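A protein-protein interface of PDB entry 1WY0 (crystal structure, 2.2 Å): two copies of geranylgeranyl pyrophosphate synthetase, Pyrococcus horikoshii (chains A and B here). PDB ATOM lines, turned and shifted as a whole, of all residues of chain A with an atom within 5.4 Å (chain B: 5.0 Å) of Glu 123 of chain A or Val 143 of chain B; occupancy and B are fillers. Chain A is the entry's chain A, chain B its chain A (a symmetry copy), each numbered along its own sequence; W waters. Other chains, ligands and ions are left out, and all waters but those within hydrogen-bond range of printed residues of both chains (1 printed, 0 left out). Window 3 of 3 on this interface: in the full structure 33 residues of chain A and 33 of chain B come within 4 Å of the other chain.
The side-chain hydroxyl (OG) of Ser 119 of chain A lies within hydrogen-bond range of the side-chain hydroxyl (OG) of Ser 146 of chain B.
OG of Ser 119 of chain A lies within hydrogen-bond range of OD1 of Asn 147 of chain B (2.6 Å).
The side-chain amide nitrogen of Asn 147 of chain B sits at hydrogen-bond distance from the side-chain carboxylate of Glu 123 of chain A (3.2 Å).
NZ of Lys 120 of chain A sits at hydrogen-bond distance from O of Leu 25 of chain A (3.1 Å).
The side-chain amino group of Lys 120 of chain A lies within salt-bridge range of the side-chain carboxylate of Glu 123 of chain A, at 3.4 Å.
The guanidinium group of Arg 127 of chain A lies within salt-bridge range of the side-chain carboxylate of Glu 123 of chain A, 3.1 Å away.
The backbone carbonyl oxygen (O) of Val 143 of chain B is in hydrogen-bond range of the side-chain amide nitrogen (ND2) of Asn 147 of chain B.
Among the printed residues, pairs that only touch across the chains: Ser 119 of chain A with Val 143 of chain B (3.8 Å), Lys 120 of chain A with Asn 147 of chain B (3.7 Å), Phe 122 of chain A with Phe 122 of chain B (3.8 Å), Phe 122 of chain A with Val 143 of chain B (3.9 Å), Glu 123 of chain A with Val 143 of chain B (3.3 Å) and Ala 126 of chain A with Leu 139 of chain B (3.9 Å).
Printed residues of chain B within 4 Å of Glu 123 of chain A: Val 143 and Asn 147.
Val 143 of chain B touches just these residues of chain A: Ser 119 (3.8 Å), Phe 122 (3.9 Å) and Glu 123 (3.3 Å).
Printed residues of chain A within 4 Å of Asn 147 of chain B: Ser 119 (2.6 Å), Lys 120 (3.7 Å) and Glu 123 (3.2 Å).
Of the printed residues of chain B, Ser 119 of chain A touches Val 143, Ser 146 and Asn 147.
Of the printed residues of chain B, Ala 126 of chain A touches Leu 139.
Of the printed residues of chain B, Lys 120 of chain A touches Asn 147.
Ala 121 of chain A touches none of the printed residues of chain B.
Val 141 of chain B touches none of the printed residues of chain A.
The nearest printed residue of chain B that does not touch Glu 123 of chain A is Lys 144 of chain B (5.3 Å).
The nearest printed residue of chain A that does not touch Val 143 of chain B is Ala 126 of chain A (5.5 Å).
Of the 11 printed residues of chain B, 5 touch a printed residue of chain A.
Printed residues of chain B that touch a printed residue of chain A: Phe 122, Leu 139, Val 143, Ser 146 and Asn 147.
Hydrophobic or aromatic side chains of chain B within 4 Å of the printed part of chain A: Phe 122, Leu 139 and Val 143.
Among the printed residues, 9 pairs touch across the chains.
Among the printed residues, no Asp or Glu carboxylate lies within 4 Å of a Lys or Arg side-chain nitrogen of the other chain.
Phe 122 of chain B touches its own counterpart, Phe 122 of chain A.
1 position is printed for both chains.
Water W1 lies within hydrogen-bond range of NZ of Lys 120 of chain A (2.9 Å) and NZ of Lys 144 of chain B (3.2 Å).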
ATOM      1  N   LEU A  25       6.977  21.359  -5.395  1.00  0.00           N
ATOM      2  CA  LEU A  25       6.392  20.349  -6.269  1.00  0.00           C
ATOM      3  C   LEU A  25       6.935  18.982  -5.847  1.00  0.00           C
ATOM      4  O   LEU A  25       6.203  17.996  -5.836  1.00  0.00           O
ATOM      5  CB  LEU A  25       6.747  20.620  -7.735  1.00  0.00           C
ATOM      6  CG  LEU A  25       5.909  21.636  -8.518  1.00  0.00           C
ATOM      7  CD1 LEU A  25       6.517  21.833  -9.883  1.00  0.00           C
ATOM      8  CD2 LEU A  25       4.470  21.146  -8.655  1.00  0.00           C
ATOM      9  N   TYR A  70       6.502  28.867 -13.395  1.00  0.00           N
ATOM     10  CA  TYR A  70       6.166  27.446 -13.432  1.00  0.00           C
ATOM     11  C   TYR A  70       6.538  26.785 -14.758  1.00  0.00           C
ATOM     12  O   TYR A  70       6.922  25.618 -14.787  1.00  0.00           O
ATOM     13  CB  TYR A  70       4.689  27.222 -13.118  1.00  0.00           C
ATOM     14  CG  TYR A  70       4.411  27.142 -11.638  1.00  0.00           C
ATOM     15  CD1 TYR A  70       3.987  28.259 -10.922  1.00  0.00           C
ATOM     16  CD2 TYR A  70       4.572  25.941 -10.948  1.00  0.00           C
ATOM     17  CE1 TYR A  70       3.725  28.181  -9.561  1.00  0.00           C
ATOM     18  CE2 TYR A  70       4.315  25.852  -9.587  1.00  0.00           C
ATOM     19  CZ  TYR A  70       3.888  26.977  -8.898  1.00  0.00           C
ATOM     20  OH  TYR A  70       3.618  26.885  -7.549  1.00  0.00           O
ATOM     21  N   SER A 119       6.402  13.701 -14.784  1.00  0.00           N
ATOM     22  CA  SER A 119       5.021  13.969 -14.430  1.00  0.00           C
ATOM     23  C   SER A 119       4.911  15.344 -13.742  1.00  0.00           C
ATOM     24  O   SER A 119       3.969  16.098 -13.983  1.00  0.00           O
ATOM     25  CB  SER A 119       4.528  12.875 -13.477  1.00  0.00           C
ATOM     26  OG  SER A 119       3.193  13.110 -13.065  1.00  0.00           O
ATOM     27  N   LYS A 120       5.875  15.670 -12.885  1.00  0.00           N
ATOM     28  CA  LYS A 120       5.675  16.952 -12.213  1.00  0.00           C
ATOM     29  C   LYS A 120       6.020  18.141 -13.119  1.00  0.00           C
ATOM     30  O   LYS A 120       5.507  19.241 -12.968  1.00  0.00           O
ATOM     31  CB  LYS A 120       6.556  16.978 -10.963  1.00  0.00           C
ATOM     32  CG  LYS A 120       6.118  15.943  -9.923  1.00  0.00           C
ATOM     33  CD  LYS A 120       5.373  16.580  -8.748  1.00  0.00           C
ATOM     34  CE  LYS A 120       4.830  15.539  -7.764  1.00  0.00           C
ATOM     35  NZ  LYS A 120       3.909  16.180  -6.828  1.00  0.00           N
ATOM     36  N   ALA A 121       6.794  17.950 -14.182  1.00  0.00           N
ATOM     37  CA  ALA A 121       7.004  19.011 -15.151  1.00  0.00           C
ATOM     38  C   ALA A 121       5.652  19.467 -15.707  1.00  0.00           C
ATOM     39  O   ALA A 121       5.420  20.661 -15.897  1.00  0.00           O
ATOM     40  CB  ALA A 121       7.901  18.517 -16.278  1.00  0.00           C
ATOM     41  N   PHE A 122       4.771  18.511 -15.986  1.00  0.00           N
ATOM     42  CA  PHE A 122       3.464  18.871 -16.514  1.00  0.00           C
ATOM     43  C   PHE A 122       2.542  19.360 -15.400  1.00  0.00           C
ATOM     44  O   PHE A 122       1.613  20.126 -15.619  1.00  0.00           O
ATOM     45  CB  PHE A 122       2.863  17.636 -17.184  1.00  0.00           C
ATOM     46  CG  PHE A 122       3.528  17.402 -18.507  1.00  0.00           C
ATOM     47  CD1 PHE A 122       3.138  18.148 -19.613  1.00  0.00           C
ATOM     48  CD2 PHE A 122       4.520  16.441 -18.624  1.00  0.00           C
ATOM     49  CE1 PHE A 122       3.750  17.931 -20.840  1.00  0.00           C
ATOM     50  CE2 PHE A 122       5.129  16.232 -19.858  1.00  0.00           C
ATOM     51  CZ  PHE A 122       4.748  16.975 -20.968  1.00  0.00           C
ATOM     52  N   GLU A 123       2.790  18.964 -14.155  1.00  0.00           N
ATOM     53  CA  GLU A 123       1.961  19.546 -13.139  1.00  0.00           C
ATOM     54  C   GLU A 123       2.365  20.983 -12.957  1.00  0.00           C
ATOM     55  O   GLU A 123       1.547  21.849 -12.677  1.00  0.00           O
ATOM     56  CB  GLU A 123       2.173  18.796 -11.837  1.00  0.00           C
ATOM     57  CG  GLU A 123       1.114  19.171 -10.809  1.00  0.00           C
ATOM     58  CD  GLU A 123       1.610  18.846  -9.421  1.00  0.00           C
ATOM     59  OE1 GLU A 123       2.213  17.801  -9.244  1.00  0.00           O
ATOM     60  OE2 GLU A 123       1.356  19.631  -8.512  1.00  0.00           O
ATOM     61  N   ALA A 124       3.636  21.282 -13.218  1.00  0.00           N
ATOM     62  CA  ALA A 124       4.137  22.657 -13.194  1.00  0.00           C
ATOM     63  C   ALA A 124       3.530  23.449 -14.349  1.00  0.00           C
ATOM     64  O   ALA A 124       3.180  24.612 -14.194  1.00  0.00           O
ATOM     65  CB  ALA A 124       5.660  22.668 -13.304  1.00  0.00           C
ATOM     66  N   VAL A 125       3.420  22.816 -15.511  1.00  0.00           N
ATOM     67  CA  VAL A 125       2.837  23.469 -16.674  1.00  0.00           C
ATOM     68  C   VAL A 125       1.388  23.851 -16.392  1.00  0.00           C
ATOM     69  O   VAL A 125       0.939  24.926 -16.776  1.00  0.00           O
ATOM     70  CB  VAL A 125       2.859  22.547 -17.907  1.00  0.00           C
ATOM     71  CG1 VAL A 125       2.063  23.171 -19.042  1.00  0.00           C
ATOM     72  CG2 VAL A 125       4.290  22.310 -18.349  1.00  0.00           C
ATOM     73  N   ALA A 126       0.659  22.960 -15.728  1.00  0.00           N
ATOM     74  CA  ALA A 126      -0.735  23.205 -15.407  1.00  0.00           C
ATOM     75  C   ALA A 126      -0.900  24.383 -14.443  1.00  0.00           C
ATOM     76  O   ALA A 126      -1.781  25.216 -14.638  1.00  0.00           O
ATOM     77  CB  ALA A 126      -1.360  21.943 -14.820  1.00  0.00           C
ATOM     78  N   ARG A 127      -0.057  24.456 -13.412  1.00  0.00           N
ATOM     79  CA  ARG A 127      -0.122  25.548 -12.435  1.00  0.00           C
ATOM     80  C   ARG A 127       0.200  26.932 -13.003  1.00  0.00           C
ATOM     81  O   ARG A 127       0.034  27.935 -12.314  1.00  0.00           O
ATOM     82  CB  ARG A 127       0.829  25.286 -11.262  1.00  0.00           C
ATOM     83  CG  ARG A 127       0.455  24.115 -10.383  1.00  0.00           C
ATOM     84  CD  ARG A 127       1.315  24.109  -9.138  1.00  0.00           C
ATOM     85  NE  ARG A 127       1.000  23.001  -8.246  1.00  0.00           N
ATOM     86  CZ  ARG A 127       1.555  22.830  -7.052  1.00  0.00           C
ATOM     87  NH1 ARG A 127       2.450  23.701  -6.606  1.00  0.00           N
ATOM     88  NH2 ARG A 127       1.228  21.782  -6.310  1.00  0.00           N
ATOM     89  N   PHE B 122       0.531  13.237 -23.237  1.00  0.00           N
ATOM     90  CA  PHE B 122       0.278  14.663 -23.096  1.00  0.00           C
ATOM     91  C   PHE B 122       0.183  15.338 -24.461  1.00  0.00           C
ATOM     92  O   PHE B 122      -0.457  16.368 -24.631  1.00  0.00           O
ATOM     93  CB  PHE B 122       1.425  15.274 -22.291  1.00  0.00           C
ATOM     94  CG  PHE B 122       1.270  14.924 -20.840  1.00  0.00           C
ATOM     95  CD1 PHE B 122       0.379  15.643 -20.052  1.00  0.00           C
ATOM     96  CD2 PHE B 122       2.017  13.894 -20.293  1.00  0.00           C
ATOM     97  CE1 PHE B 122       0.237  15.323 -18.709  1.00  0.00           C
ATOM     98  CE2 PHE B 122       1.866  13.578 -18.945  1.00  0.00           C
ATOM     99  CZ  PHE B 122       0.976  14.291 -18.150  1.00  0.00           C
ATOM    100  N   VAL B 138      -8.819  18.753 -17.216  1.00  0.00           N
ATOM    101  CA  VAL B 138      -8.550  17.384 -17.646  1.00  0.00           C
ATOM    102  C   VAL B 138      -7.056  17.110 -17.471  1.00  0.00           C
ATOM    103  O   VAL B 138      -6.665  16.063 -16.969  1.00  0.00           O
ATOM    104  CB  VAL B 138      -8.944  17.168 -19.130  1.00  0.00           C
ATOM    105  CG1 VAL B 138      -8.429  15.818 -19.624  1.00  0.00           C
ATOM    106  CG2 VAL B 138     -10.462  17.219 -19.280  1.00  0.00           C
ATOM    107  N   LEU B 139      -6.230  18.063 -17.888  1.00  0.00           N
ATOM    108  CA  LEU B 139      -4.785  17.936 -17.766  1.00  0.00           C
ATOM    109  C   LEU B 139      -4.415  17.711 -16.309  1.00  0.00           C
ATOM    110  O   LEU B 139      -3.545  16.898 -16.008  1.00  0.00           O
ATOM    111  CB  LEU B 139      -4.092  19.202 -18.270  1.00  0.00           C
ATOM    112  CG  LEU B 139      -2.581  19.333 -18.024  1.00  0.00           C
ATOM    113  CD1 LEU B 139      -1.831  18.287 -18.816  1.00  0.00           C
ATOM    114  CD2 LEU B 139      -2.119  20.715 -18.420  1.00  0.00           C
ATOM    115  N   GLU B 140      -5.089  18.422 -15.408  1.00  0.00           N
ATOM    116  CA  GLU B 140      -4.812  18.321 -13.982  1.00  0.00           C
ATOM    117  C   GLU B 140      -5.275  17.025 -13.322  1.00  0.00           C
ATOM    118  O   GLU B 140      -4.736  16.623 -12.289  1.00  0.00           O
ATOM    119  CB  GLU B 140      -5.399  19.531 -13.244  1.00  0.00           C
ATOM    120  CG  GLU B 140      -5.440  19.372 -11.736  1.00  0.00           C
ATOM    121  CD  GLU B 140      -5.668  20.686 -11.003  1.00  0.00           C
ATOM    122  OE1 GLU B 140      -6.342  21.580 -11.565  1.00  0.00           O
ATOM    123  OE2 GLU B 140      -5.182  20.818  -9.856  1.00  0.00           O
ATOM    124  N   VAL B 141      -6.277  16.379 -13.903  1.00  0.00           N
ATOM    125  CA  VAL B 141      -6.764  15.116 -13.367  1.00  0.00           C
ATOM    126  C   VAL B 141      -5.775  14.030 -13.783  1.00  0.00           C
ATOM    127  O   VAL B 141      -5.433  13.139 -13.010  1.00  0.00           O
ATOM    128  CB  VAL B 141      -8.146  14.741 -13.950  1.00  0.00           C
ATOM    129  CG1 VAL B 141      -8.383  13.248 -13.792  1.00  0.00           C
ATOM    130  CG2 VAL B 141      -9.247  15.518 -13.245  1.00  0.00           C
ATOM    131  N   ILE B 142      -5.322  14.124 -15.022  1.00  0.00           N
ATOM    132  CA  ILE B 142      -4.392  13.156 -15.566  1.00  0.00           C
ATOM    133  C   ILE B 142      -3.036  13.270 -14.884  1.00  0.00           C
ATOM    134  O   ILE B 142      -2.387  12.273 -14.623  1.00  0.00           O
ATOM    135  CB  ILE B 142      -4.272  13.342 -17.092  1.00  0.00           C
ATOM    136  CG1 ILE B 142      -5.596  12.914 -17.754  1.00  0.00           C
ATOM    137  CG2 ILE B 142      -3.093  12.550 -17.634  1.00  0.00           C
ATOM    138  CD1 ILE B 142      -5.643  13.085 -19.284  1.00  0.00           C
ATOM    139  N   VAL B 143      -2.626  14.491 -14.569  1.00  0.00           N
ATOM    140  CA  VAL B 143      -1.358  14.698 -13.903  1.00  0.00           C
ATOM    141  C   VAL B 143      -1.384  14.128 -12.489  1.00  0.00           C
ATOM    142  O   VAL B 143      -0.454  13.435 -12.076  1.00  0.00           O
ATOM    143  CB  VAL B 143      -1.002  16.192 -13.865  1.00  0.00           C
ATOM    144  CG1 VAL B 143      -0.083  16.486 -12.694  1.00  0.00           C
ATOM    145  CG2 VAL B 143      -0.327  16.583 -15.173  1.00  0.00           C
ATOM    146  N   LYS B 144      -2.439  14.402 -11.734  1.00  0.00           N
ATOM    147  CA  LYS B 144      -2.498  13.868 -10.378  1.00  0.00           C
ATOM    148  C   LYS B 144      -2.579  12.346 -10.354  1.00  0.00           C
ATOM    149  O   LYS B 144      -2.065  11.716  -9.437  1.00  0.00           O
ATOM    150  CB  LYS B 144      -3.678  14.448  -9.610  1.00  0.00           C
ATOM    151  CG  LYS B 144      -4.089  13.613  -8.388  1.00  0.00           C
ATOM    152  CD  LYS B 144      -3.220  13.889  -7.150  1.00  0.00           C
ATOM    153  CE  LYS B 144      -1.868  13.156  -7.163  1.00  0.00           C
ATOM    154  NZ  LYS B 144      -0.744  14.105  -6.869  1.00  0.00           N
ATOM    155  N   ALA B 145      -3.227  11.747 -11.344  1.00  0.00           N
ATOM    156  CA  ALA B 145      -3.324  10.294 -11.381  1.00  0.00           C
ATOM    157  C   ALA B 145      -1.950   9.753 -11.757  1.00  0.00           C
ATOM    158  O   ALA B 145      -1.526   8.704 -11.278  1.00  0.00           O
ATOM    159  CB  ALA B 145      -4.372   9.850 -12.401  1.00  0.00           C
ATOM    160  N   SER B 146      -1.258  10.480 -12.624  1.00  0.00           N
ATOM    161  CA  SER B 146       0.087  10.096 -13.033  1.00  0.00           C
ATOM    162  C   SER B 146       0.982  10.027 -11.787  1.00  0.00           C
ATOM    163  O   SER B 146       1.662   9.032 -11.559  1.00  0.00           O
ATOM    164  CB  SER B 146       0.651  11.123 -14.010  1.00  0.00           C
ATOM    165  OG  SER B 146       2.009  10.845 -14.298  1.00  0.00           O
ATOM    166  N   ASN B 147       0.966  11.084 -10.981  1.00  0.00           N
ATOM    167  CA  ASN B 147       1.774  11.122  -9.769  1.00  0.00           C
ATOM    168  C   ASN B 147       1.414   9.962  -8.817  1.00  0.00           C
ATOM    169  O   ASN B 147       2.299   9.299  -8.278  1.00  0.00           O
ATOM    170  CB  ASN B 147       1.604  12.465  -9.037  1.00  0.00           C
ATOM    171  CG  ASN B 147       2.141  13.655  -9.831  1.00  0.00           C
ATOM    172  OD1 ASN B 147       3.194  13.579 -10.476  1.00  0.00           O
ATOM    173  ND2 ASN B 147       1.424  14.772  -9.764  1.00  0.00           N
HETATM  174  O   HOH W   1       2.120  14.351  -5.441  1.00  0.00           O
